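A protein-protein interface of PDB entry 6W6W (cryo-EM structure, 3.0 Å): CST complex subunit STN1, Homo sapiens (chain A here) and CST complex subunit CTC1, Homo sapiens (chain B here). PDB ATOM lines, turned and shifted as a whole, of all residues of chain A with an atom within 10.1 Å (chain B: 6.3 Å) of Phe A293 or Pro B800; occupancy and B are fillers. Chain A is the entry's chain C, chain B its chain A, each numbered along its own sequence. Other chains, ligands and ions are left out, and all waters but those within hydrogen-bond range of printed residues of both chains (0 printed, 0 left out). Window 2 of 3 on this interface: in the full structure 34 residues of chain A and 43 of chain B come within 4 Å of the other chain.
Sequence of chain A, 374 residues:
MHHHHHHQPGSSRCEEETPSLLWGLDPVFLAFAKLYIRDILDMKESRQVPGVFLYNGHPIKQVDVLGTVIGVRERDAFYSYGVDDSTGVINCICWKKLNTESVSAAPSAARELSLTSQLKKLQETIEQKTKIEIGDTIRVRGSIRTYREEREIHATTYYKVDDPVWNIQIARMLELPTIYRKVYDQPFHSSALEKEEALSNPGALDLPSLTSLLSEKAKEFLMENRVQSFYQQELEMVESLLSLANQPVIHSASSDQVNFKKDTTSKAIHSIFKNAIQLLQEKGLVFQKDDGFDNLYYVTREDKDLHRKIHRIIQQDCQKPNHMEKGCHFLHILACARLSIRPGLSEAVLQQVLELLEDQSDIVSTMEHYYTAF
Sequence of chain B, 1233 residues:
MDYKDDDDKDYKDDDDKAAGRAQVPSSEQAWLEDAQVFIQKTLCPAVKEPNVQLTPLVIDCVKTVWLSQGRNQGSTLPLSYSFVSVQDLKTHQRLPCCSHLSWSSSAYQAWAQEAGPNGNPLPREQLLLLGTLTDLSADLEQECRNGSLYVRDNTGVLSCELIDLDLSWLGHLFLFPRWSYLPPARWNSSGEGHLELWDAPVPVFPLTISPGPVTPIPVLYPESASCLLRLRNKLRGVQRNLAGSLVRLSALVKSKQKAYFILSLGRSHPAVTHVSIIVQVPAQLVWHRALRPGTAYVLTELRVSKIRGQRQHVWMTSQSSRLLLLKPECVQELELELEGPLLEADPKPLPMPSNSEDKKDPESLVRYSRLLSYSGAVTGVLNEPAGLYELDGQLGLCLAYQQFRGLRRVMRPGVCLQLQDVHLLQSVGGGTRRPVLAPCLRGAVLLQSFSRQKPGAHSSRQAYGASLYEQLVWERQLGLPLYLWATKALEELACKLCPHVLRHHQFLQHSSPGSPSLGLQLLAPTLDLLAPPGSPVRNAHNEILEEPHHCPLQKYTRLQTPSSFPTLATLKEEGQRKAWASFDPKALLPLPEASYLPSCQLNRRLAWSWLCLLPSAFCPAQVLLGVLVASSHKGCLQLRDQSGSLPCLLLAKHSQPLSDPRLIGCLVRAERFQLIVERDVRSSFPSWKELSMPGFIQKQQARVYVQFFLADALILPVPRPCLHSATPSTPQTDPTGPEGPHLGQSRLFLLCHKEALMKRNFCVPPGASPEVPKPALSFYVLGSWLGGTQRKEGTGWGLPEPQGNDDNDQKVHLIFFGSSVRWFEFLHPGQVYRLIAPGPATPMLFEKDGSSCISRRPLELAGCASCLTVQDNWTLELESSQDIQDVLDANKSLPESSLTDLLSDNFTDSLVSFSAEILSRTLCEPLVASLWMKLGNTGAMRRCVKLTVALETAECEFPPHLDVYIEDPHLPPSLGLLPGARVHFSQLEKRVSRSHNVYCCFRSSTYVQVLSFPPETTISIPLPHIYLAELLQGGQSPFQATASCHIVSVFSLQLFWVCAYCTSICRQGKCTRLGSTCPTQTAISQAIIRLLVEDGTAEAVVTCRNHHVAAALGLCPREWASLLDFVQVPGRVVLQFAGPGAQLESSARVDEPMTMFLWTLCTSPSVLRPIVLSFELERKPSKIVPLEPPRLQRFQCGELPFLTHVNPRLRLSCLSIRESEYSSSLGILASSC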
ATOM      1  N   SER A 229      13.041  34.289 -24.941  1.00  0.00           N
ATOM      2  CA  SER A 229      12.114  34.191 -23.827  1.00  0.00           C
ATOM      3  C   SER A 229      12.457  35.247 -22.789  1.00  0.00           C
ATOM      4  O   SER A 229      13.591  35.722 -22.707  1.00  0.00           O
ATOM      5  CB  SER A 229      12.145  32.801 -23.181  1.00  0.00           C
ATOM      6  OG  SER A 229      13.390  32.557 -22.551  1.00  0.00           O
ATOM      7  N   PHE A 230      11.460  35.605 -21.986  1.00  0.00           N
ATOM      8  CA  PHE A 230      11.660  36.583 -20.930  1.00  0.00           C
ATOM      9  C   PHE A 230      10.717  36.273 -19.780  1.00  0.00           C
ATOM     10  O   PHE A 230       9.749  35.522 -19.926  1.00  0.00           O
ATOM     11  CB  PHE A 230      11.454  38.024 -21.434  1.00  0.00           C
ATOM     12  CG  PHE A 230      10.067  38.310 -21.960  1.00  0.00           C
ATOM     13  CD1 PHE A 230       9.741  38.038 -23.280  1.00  0.00           C
ATOM     14  CD2 PHE A 230       9.102  38.884 -21.144  1.00  0.00           C
ATOM     15  CE1 PHE A 230       8.474  38.306 -23.766  1.00  0.00           C
ATOM     16  CE2 PHE A 230       7.835  39.151 -21.622  1.00  0.00           C
ATOM     17  CZ  PHE A 230       7.522  38.864 -22.935  1.00  0.00           C
ATOM     18  N   TYR A 231      11.013  36.865 -18.632  1.00  0.00           N
ATOM     19  CA  TYR A 231      10.129  36.830 -17.480  1.00  0.00           C
ATOM     20  C   TYR A 231       9.394  38.157 -17.367  1.00  0.00           C
ATOM     21  O   TYR A 231       9.769  39.154 -17.987  1.00  0.00           O
ATOM     22  CB  TYR A 231      10.910  36.550 -16.195  1.00  0.00           C
ATOM     23  CG  TYR A 231      11.409  35.133 -16.083  1.00  0.00           C
ATOM     24  CD1 TYR A 231      12.604  34.749 -16.677  1.00  0.00           C
ATOM     25  CD2 TYR A 231      10.689  34.178 -15.381  1.00  0.00           C
ATOM     26  CE1 TYR A 231      13.064  33.454 -16.578  1.00  0.00           C
ATOM     27  CE2 TYR A 231      11.141  32.881 -15.276  1.00  0.00           C
ATOM     28  CZ  TYR A 231      12.328  32.526 -15.877  1.00  0.00           C
ATOM     29  OH  TYR A 231      12.785  31.235 -15.777  1.00  0.00           O
ATOM     30  N   GLN A 232       8.328  38.158 -16.566  1.00  0.00           N
ATOM     31  CA  GLN A 232       7.550  39.377 -16.388  1.00  0.00           C
ATOM     32  C   GLN A 232       8.314  40.413 -15.577  1.00  0.00           C
ATOM     33  O   GLN A 232       8.211  41.613 -15.852  1.00  0.00           O
ATOM     34  CB  GLN A 232       6.217  39.057 -15.718  1.00  0.00           C
ATOM     35  CG  GLN A 232       5.205  40.182 -15.787  1.00  0.00           C
ATOM     36  CD  GLN A 232       4.301  40.218 -14.577  1.00  0.00           C
ATOM     37  OE1 GLN A 232       3.927  39.179 -14.037  1.00  0.00           O
ATOM     38  NE2 GLN A 232       3.948  41.421 -14.140  1.00  0.00           N
ATOM     39  N   GLN A 233       9.105  39.972 -14.599  1.00  0.00           N
ATOM     40  CA  GLN A 233       9.884  40.879 -13.770  1.00  0.00           C
ATOM     41  C   GLN A 233      11.102  41.447 -14.483  1.00  0.00           C
ATOM     42  O   GLN A 233      11.727  42.373 -13.957  1.00  0.00           O
ATOM     43  CB  GLN A 233      10.328  40.168 -12.494  1.00  0.00           C
ATOM     44  CG  GLN A 233       9.192  39.856 -11.544  1.00  0.00           C
ATOM     45  CD  GLN A 233       8.673  38.448 -11.707  1.00  0.00           C
ATOM     46  OE1 GLN A 233       8.349  38.019 -12.813  1.00  0.00           O
ATOM     47  NE2 GLN A 233       8.588  37.719 -10.604  1.00  0.00           N
ATOM     48  N   PHE A 287       3.545  33.698 -26.128  1.00  0.00           N
ATOM     49  CA  PHE A 287       2.849  32.527 -25.613  1.00  0.00           C
ATOM     50  C   PHE A 287       3.652  31.949 -24.459  1.00  0.00           C
ATOM     51  O   PHE A 287       4.775  32.374 -24.181  1.00  0.00           O
ATOM     52  CB  PHE A 287       2.615  31.478 -26.709  1.00  0.00           C
ATOM     53  CG  PHE A 287       3.826  30.643 -27.034  1.00  0.00           C
ATOM     54  CD1 PHE A 287       4.872  31.169 -27.771  1.00  0.00           C
ATOM     55  CD2 PHE A 287       3.908  29.324 -26.616  1.00  0.00           C
ATOM     56  CE1 PHE A 287       5.977  30.400 -28.085  1.00  0.00           C
ATOM     57  CE2 PHE A 287       5.013  28.550 -26.919  1.00  0.00           C
ATOM     58  CZ  PHE A 287       6.048  29.089 -27.653  1.00  0.00           C
ATOM     59  N   GLN A 288       3.055  30.968 -23.789  1.00  0.00           N
ATOM     60  CA  GLN A 288       3.684  30.305 -22.660  1.00  0.00           C
ATOM     61  C   GLN A 288       3.199  28.866 -22.585  1.00  0.00           C
ATOM     62  O   GLN A 288       2.068  28.549 -22.960  1.00  0.00           O
ATOM     63  CB  GLN A 288       3.390  31.034 -21.346  1.00  0.00           C
ATOM     64  CG  GLN A 288       1.942  31.445 -21.176  1.00  0.00           C
ATOM     65  CD  GLN A 288       1.603  31.783 -19.741  1.00  0.00           C
ATOM     66  OE1 GLN A 288       2.471  31.784 -18.870  1.00  0.00           O
ATOM     67  NE2 GLN A 288       0.332  32.070 -19.485  1.00  0.00           N
ATOM     68  N   LYS A 289       4.071  27.994 -22.093  1.00  0.00           N
ATOM     69  CA  LYS A 289       3.768  26.581 -21.937  1.00  0.00           C
ATOM     70  C   LYS A 289       3.647  26.242 -20.458  1.00  0.00           C
ATOM     71  O   LYS A 289       4.038  27.019 -19.583  1.00  0.00           O
ATOM     72  CB  LYS A 289       4.839  25.709 -22.605  1.00  0.00           C
ATOM     73  CG  LYS A 289       6.243  25.937 -22.082  1.00  0.00           C
ATOM     74  CD  LYS A 289       7.285  25.476 -23.086  1.00  0.00           C
ATOM     75  CE  LYS A 289       7.283  26.355 -24.322  1.00  0.00           C
ATOM     76  NZ  LYS A 289       8.592  26.312 -25.030  1.00  0.00           N
ATOM     77  N   ASP A 290       3.087  25.067 -20.188  1.00  0.00           N
ATOM     78  CA  ASP A 290       2.860  24.607 -18.821  1.00  0.00           C
ATOM     79  C   ASP A 290       4.198  24.190 -18.221  1.00  0.00           C
ATOM     80  O   ASP A 290       4.721  23.116 -18.524  1.00  0.00           O
ATOM     81  CB  ASP A 290       1.860  23.455 -18.817  1.00  0.00           C
ATOM     82  CG  ASP A 290       1.300  23.160 -17.436  1.00  0.00           C
ATOM     83  OD1 ASP A 290       1.674  23.854 -16.466  1.00  0.00           O
ATOM     84  OD2 ASP A 290       0.477  22.229 -17.320  1.00  0.00           O
ATOM     85  N   ASP A 291       4.758  25.043 -17.360  1.00  0.00           N
ATOM     86  CA  ASP A 291       6.075  24.801 -16.791  1.00  0.00           C
ATOM     87  C   ASP A 291       6.174  25.035 -15.290  1.00  0.00           C
ATOM     88  O   ASP A 291       7.245  24.795 -14.724  1.00  0.00           O
ATOM     89  CB  ASP A 291       7.129  25.669 -17.495  1.00  0.00           C
ATOM     90  CG  ASP A 291       6.634  27.074 -17.784  1.00  0.00           C
ATOM     91  OD1 ASP A 291       6.974  27.613 -18.858  1.00  0.00           O
ATOM     92  OD2 ASP A 291       5.901  27.641 -16.949  1.00  0.00           O
ATOM     93  N   GLY A 292       5.113  25.492 -14.632  1.00  0.00           N
ATOM     94  CA  GLY A 292       5.142  25.655 -13.191  1.00  0.00           C
ATOM     95  C   GLY A 292       4.938  27.073 -12.700  1.00  0.00           C
ATOM     96  O   GLY A 292       4.230  27.288 -11.712  1.00  0.00           O
ATOM     97  N   PHE A 293       5.548  28.051 -13.364  1.00  0.00           N
ATOM     98  CA  PHE A 293       5.357  29.453 -13.024  1.00  0.00           C
ATOM     99  C   PHE A 293       4.669  30.194 -14.162  1.00  0.00           C
ATOM    100  O   PHE A 293       4.755  29.799 -15.328  1.00  0.00           O
ATOM    101  CB  PHE A 293       6.681  30.139 -12.671  1.00  0.00           C
ATOM    102  CG  PHE A 293       7.874  29.589 -13.396  1.00  0.00           C
ATOM    103  CD1 PHE A 293       8.777  28.772 -12.733  1.00  0.00           C
ATOM    104  CD2 PHE A 293       8.094  29.880 -14.727  1.00  0.00           C
ATOM    105  CE1 PHE A 293       9.878  28.264 -13.379  1.00  0.00           C
ATOM    106  CE2 PHE A 293       9.194  29.369 -15.382  1.00  0.00           C
ATOM    107  CZ  PHE A 293      10.087  28.560 -14.705  1.00  0.00           C
ATOM    108  N   ASP A 294       3.988  31.281 -13.807  1.00  0.00           N
ATOM    109  CA  ASP A 294       3.077  31.973 -14.706  1.00  0.00           C
ATOM    110  C   ASP A 294       3.637  33.286 -15.237  1.00  0.00           C
ATOM    111  O   ASP A 294       2.897  34.057 -15.854  1.00  0.00           O
ATOM    112  CB  ASP A 294       1.747  32.227 -13.998  1.00  0.00           C
ATOM    113  CG  ASP A 294       1.020  30.943 -13.650  1.00  0.00           C
ATOM    114  OD1 ASP A 294       1.189  29.946 -14.382  1.00  0.00           O
ATOM    115  OD2 ASP A 294       0.286  30.929 -12.639  1.00  0.00           O
ATOM    116  N   ASN A 295       4.919  33.564 -15.011  1.00  0.00           N
ATOM    117  CA  ASN A 295       5.531  34.801 -15.471  1.00  0.00           C
ATOM    118  C   ASN A 295       6.472  34.603 -16.648  1.00  0.00           C
ATOM    119  O   ASN A 295       6.979  35.590 -17.188  1.00  0.00           O
ATOM    120  CB  ASN A 295       6.283  35.478 -14.321  1.00  0.00           C
ATOM    121  CG  ASN A 295       7.069  34.497 -13.485  1.00  0.00           C
ATOM    122  OD1 ASN A 295       7.132  33.311 -13.799  1.00  0.00           O
ATOM    123  ND2 ASN A 295       7.670  34.986 -12.407  1.00  0.00           N
ATOM    124  N   LEU A 296       6.719  33.363 -17.063  1.00  0.00           N
ATOM    125  CA  LEU A 296       7.610  33.085 -18.181  1.00  0.00           C
ATOM    126  C   LEU A 296       6.835  33.157 -19.489  1.00  0.00           C
ATOM    127  O   LEU A 296       5.753  32.576 -19.609  1.00  0.00           O
ATOM    128  CB  LEU A 296       8.256  31.709 -18.032  1.00  0.00           C
ATOM    129  CG  LEU A 296       9.341  31.390 -19.058  1.00  0.00           C
ATOM    130  CD1 LEU A 296      10.470  32.390 -18.951  1.00  0.00           C
ATOM    131  CD2 LEU A 296       9.863  29.978 -18.890  1.00  0.00           C
ATOM    132  N   TYR A 297       7.394  33.863 -20.467  1.00  0.00           N
ATOM    133  CA  TYR A 297       6.777  34.007 -21.775  1.00  0.00           C
ATOM    134  C   TYR A 297       7.813  33.754 -22.861  1.00  0.00           C
ATOM    135  O   TYR A 297       9.014  33.926 -22.654  1.00  0.00           O
ATOM    136  CB  TYR A 297       6.161  35.398 -21.956  1.00  0.00           C
ATOM    137  CG  TYR A 297       5.011  35.673 -21.020  1.00  0.00           C
ATOM    138  CD1 TYR A 297       3.775  35.072 -21.217  1.00  0.00           C
ATOM    139  CD2 TYR A 297       5.162  36.526 -19.936  1.00  0.00           C
ATOM    140  CE1 TYR A 297       2.718  35.317 -20.362  1.00  0.00           C
ATOM    141  CE2 TYR A 297       4.113  36.776 -19.074  1.00  0.00           C
ATOM    142  CZ  TYR A 297       2.895  36.170 -19.293  1.00  0.00           C
ATOM    143  OH  TYR A 297       1.848  36.420 -18.437  1.00  0.00           O
ATOM    144  N   TYR A 298       7.324  33.342 -24.028  1.00  0.00           N
ATOM    145  CA  TYR A 298       8.158  33.093 -25.194  1.00  0.00           C
ATOM    146  C   TYR A 298       7.603  33.883 -26.368  1.00  0.00           C
ATOM    147  O   TYR A 298       6.385  33.995 -26.524  1.00  0.00           O
ATOM    148  CB  TYR A 298       8.201  31.602 -25.564  1.00  0.00           C
ATOM    149  CG  TYR A 298       8.738  30.665 -24.504  1.00  0.00           C
ATOM    150  CD1 TYR A 298       7.923  30.196 -23.479  1.00  0.00           C
ATOM    151  CD2 TYR A 298      10.049  30.215 -24.554  1.00  0.00           C
ATOM    152  CE1 TYR A 298       8.409  29.327 -22.520  1.00  0.00           C
ATOM    153  CE2 TYR A 298      10.544  29.346 -23.599  1.00  0.00           C
ATOM    154  CZ  TYR A 298       9.719  28.906 -22.586  1.00  0.00           C
ATOM    155  OH  TYR A 298      10.210  28.040 -21.637  1.00  0.00           O
ATOM    156  N   LEU B 748      15.258  30.199  -8.693  1.00  0.00           N
ATOM    157  CA  LEU B 748      15.760  31.232  -9.587  1.00  0.00           C
ATOM    158  C   LEU B 748      15.498  32.612  -9.005  1.00  0.00           C
ATOM    159  O   LEU B 748      14.532  32.821  -8.268  1.00  0.00           O
ATOM    160  CB  LEU B 748      15.108  31.144 -10.968  1.00  0.00           C
ATOM    161  CG  LEU B 748      15.547  30.111 -12.005  1.00  0.00           C
ATOM    162  CD1 LEU B 748      15.058  28.724 -11.664  1.00  0.00           C
ATOM    163  CD2 LEU B 748      15.051  30.517 -13.373  1.00  0.00           C
ATOM    164  N   LEU B 786      11.776  34.314  -8.756  1.00  0.00           N
ATOM    165  CA  LEU B 786      10.960  34.104  -9.940  1.00  0.00           C
ATOM    166  C   LEU B 786      10.086  32.864  -9.845  1.00  0.00           C
ATOM    167  O   LEU B 786       9.361  32.562 -10.796  1.00  0.00           O
ATOM    168  CB  LEU B 786      11.848  34.012 -11.180  1.00  0.00           C
ATOM    169  CG  LEU B 786      12.701  35.242 -11.467  1.00  0.00           C
ATOM    170  CD1 LEU B 786      13.610  34.987 -12.647  1.00  0.00           C
ATOM    171  CD2 LEU B 786      11.819  36.441 -11.726  1.00  0.00           C
ATOM    172  N   GLY B 787      10.134  32.145  -8.733  1.00  0.00           N
ATOM    173  CA  GLY B 787       9.311  30.960  -8.590  1.00  0.00           C
ATOM    174  C   GLY B 787       9.605  30.270  -7.281  1.00  0.00           C
ATOM    175  O   GLY B 787      10.405  30.741  -6.465  1.00  0.00           O
ATOM    176  N   GLY B 788       8.938  29.138  -7.086  1.00  0.00           N
ATOM    177  CA  GLY B 788       9.118  28.350  -5.890  1.00  0.00           C
ATOM    178  C   GLY B 788      10.354  27.480  -5.955  1.00  0.00           C
ATOM    179  O   GLY B 788      11.110  27.480  -6.924  1.00  0.00           O
ATOM    180  N   THR B 789      10.552  26.714  -4.888  1.00  0.00           N
ATOM    181  CA  THR B 789      11.720  25.851  -4.773  1.00  0.00           C
ATOM    182  C   THR B 789      11.548  24.632  -5.669  1.00  0.00           C
ATOM    183  O   THR B 789      10.573  23.885  -5.532  1.00  0.00           O
ATOM    184  CB  THR B 789      11.927  25.433  -3.320  1.00  0.00           C
ATOM    185  OG1 THR B 789      12.321  26.572  -2.548  1.00  0.00           O
ATOM    186  CG2 THR B 789      13.003  24.372  -3.220  1.00  0.00           C
ATOM    187  N   GLN B 790      12.487  24.434  -6.587  1.00  0.00           N
ATOM    188  CA  GLN B 790      12.500  23.276  -7.467  1.00  0.00           C
ATOM    189  C   GLN B 790      13.426  22.210  -6.907  1.00  0.00           C
ATOM    190  O   GLN B 790      14.470  22.522  -6.331  1.00  0.00           O
ATOM    191  CB  GLN B 790      12.956  23.662  -8.872  1.00  0.00           C
ATOM    192  CG  GLN B 790      11.989  24.538  -9.623  1.00  0.00           C
ATOM    193  CD  GLN B 790      12.612  25.156 -10.850  1.00  0.00           C
ATOM    194  OE1 GLN B 790      13.829  25.312 -10.928  1.00  0.00           O
ATOM    195  NE2 GLN B 790      11.785  25.500 -11.823  1.00  0.00           N
ATOM    196  N   ARG B 791      13.042  20.951  -7.078  1.00  0.00           N
ATOM    197  CA  ARG B 791      13.863  19.828  -6.654  1.00  0.00           C
ATOM    198  C   ARG B 791      14.480  19.147  -7.867  1.00  0.00           C
ATOM    199  O   ARG B 791      13.902  19.135  -8.956  1.00  0.00           O
ATOM    200  CB  ARG B 791      13.044  18.821  -5.845  1.00  0.00           C
ATOM    201  CG  ARG B 791      12.877  19.207  -4.385  1.00  0.00           C
ATOM    202  CD  ARG B 791      12.263  18.081  -3.572  1.00  0.00           C
ATOM    203  NE  ARG B 791      13.257  17.090  -3.171  1.00  0.00           N
ATOM    204  CZ  ARG B 791      13.246  15.820  -3.560  1.00  0.00           C
ATOM    205  NH1 ARG B 791      12.289  15.379  -4.364  1.00  0.00           N
ATOM    206  NH2 ARG B 791      14.192  14.989  -3.144  1.00  0.00           N
ATOM    207  N   GLY B 798      12.469  19.943 -11.381  1.00  0.00           N
ATOM    208  CA  GLY B 798      11.054  19.674 -11.501  1.00  0.00           C
ATOM    209  C   GLY B 798      10.218  20.936 -11.574  1.00  0.00           C
ATOM    210  O   GLY B 798      10.655  21.999 -12.018  1.00  0.00           O
ATOM    211  N   LEU B 799       8.985  20.802 -11.136  1.00  0.00           N
ATOM    212  CA  LEU B 799       8.096  21.950 -11.094  1.00  0.00           C
ATOM    213  C   LEU B 799       8.220  22.646  -9.740  1.00  0.00           C
ATOM    214  O   LEU B 799       8.450  21.987  -8.724  1.00  0.00           O
ATOM    215  CB  LEU B 799       6.649  21.515 -11.334  1.00  0.00           C
ATOM    216  CG  LEU B 799       6.344  20.826 -12.667  1.00  0.00           C
ATOM    217  CD1 LEU B 799       4.845  20.745 -12.889  1.00  0.00           C
ATOM    218  CD2 LEU B 799       7.016  21.537 -13.832  1.00  0.00           C
ATOM    219  N   PRO B 800       8.094  23.971  -9.701  1.00  0.00           N
ATOM    220  CA  PRO B 800       8.262  24.688  -8.434  1.00  0.00           C
ATOM    221  C   PRO B 800       7.082  24.483  -7.500  1.00  0.00           C
ATOM    222  O   PRO B 800       5.953  24.222  -7.918  1.00  0.00           O
ATOM    223  CB  PRO B 800       8.369  26.155  -8.867  1.00  0.00           C
ATOM    224  CG  PRO B 800       8.658  26.112 -10.322  1.00  0.00           C
ATOM    225  CD  PRO B 800       7.974  24.900 -10.833  1.00  0.00           C
ATOM    226  N   GLU B 801       7.370  24.601  -6.207  1.00  0.00           N
ATOM    227  CA  GLU B 801       6.328  24.574  -5.198  1.00  0.00           C
ATOM    228  C   GLU B 801       5.488  25.850  -5.294  1.00  0.00           C
ATOM    229  O   GLU B 801       5.962  26.874  -5.796  1.00  0.00           O
ATOM    230  CB  GLU B 801       6.951  24.405  -3.810  1.00  0.00           C
ATOM    231  CG  GLU B 801       7.477  25.674  -3.162  1.00  0.00           C
ATOM    232  CD  GLU B 801       7.950  25.444  -1.739  1.00  0.00           C
ATOM    233  OE1 GLU B 801       8.057  24.270  -1.329  1.00  0.00           O
ATOM    234  OE2 GLU B 801       8.218  26.436  -1.030  1.00  0.00           O
ATOM    235  N   PRO B 802       4.217  25.796  -4.884  1.00  0.00           N
ATOM    236  CA  PRO B 802       3.358  26.985  -4.994  1.00  0.00           C
ATOM    237  C   PRO B 802       3.807  28.105  -4.067  1.00  0.00           C
ATOM    238  O   PRO B 802       4.000  27.906  -2.866  1.00  0.00           O
ATOM    239  CB  PRO B 802       1.972  26.454  -4.611  1.00  0.00           C
ATOM    240  CG  PRO B 802       2.031  25.008  -4.930  1.00  0.00           C
ATOM    241  CD  PRO B 802       3.424  24.591  -4.581  1.00  0.00           C
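The side-chain amide nitrogen (ND2) of Asn A295 lies within hydrogen-bond range of the backbone carbonyl oxygen (O) of Leu B786 (3.4 Å).
The backbone carbonyl oxygen (O) of Leu B748 lies within hydrogen-bond range of the backbone NH (N) of Leu B786 (3.2 Å). The backbone carbonyl oxygen (O) of Asn A295 lies within hydrogen-bond range of the backbone NH (N) of Gln A232, 3.0 Å away. The side-chain amide oxygen of Gln A233 sits at hydrogen-bond distance from the side-chain amide nitrogen of Asn A295.
Among the printed residues, pairs that only touch across the chains: Tyr A231 with Leu B748, Gln A233 with Leu B786, Asp A291 with Leu B799, Asp A291 with Pro B800, Gly A292 with Pro B800, Phe A293 with Gln B790 and Phe A293 with Pro B800.
Phe A293 touches just these residues of chain B: Gln B790 and Pro B800. Pro B800 touches three residues of chain A. No residue of chain A comes within 4 Å of Gly B788. Printed residues of chain B within 4 Å of Tyr A231: Leu B748. Printed residues of chain B within 4 Å of Gln A233: Leu B786. Printed residues of chain A within 4 Å of Leu B786: Gln A233 (3.7 Å) and Asn A295 (3.4 Å). Leu A296 touches none of the printed residues of chain B. Phe A287 touches none of the printed residues of chain B.
Of the 12 printed residues of chain B, 5 touch a printed residue of chain A. Hydrophobic or aromatic side chains of chain B within 4 Å of the printed part of chain A: Leu B748, Leu B786, Leu B799 and Pro B800. Of the 17 printed residues of chain A, 6 touch a printed residue of chain B. Hydrophobic or aromatic side chains of chain A that line the printed part of chain B: Tyr A231 and Phe A293.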
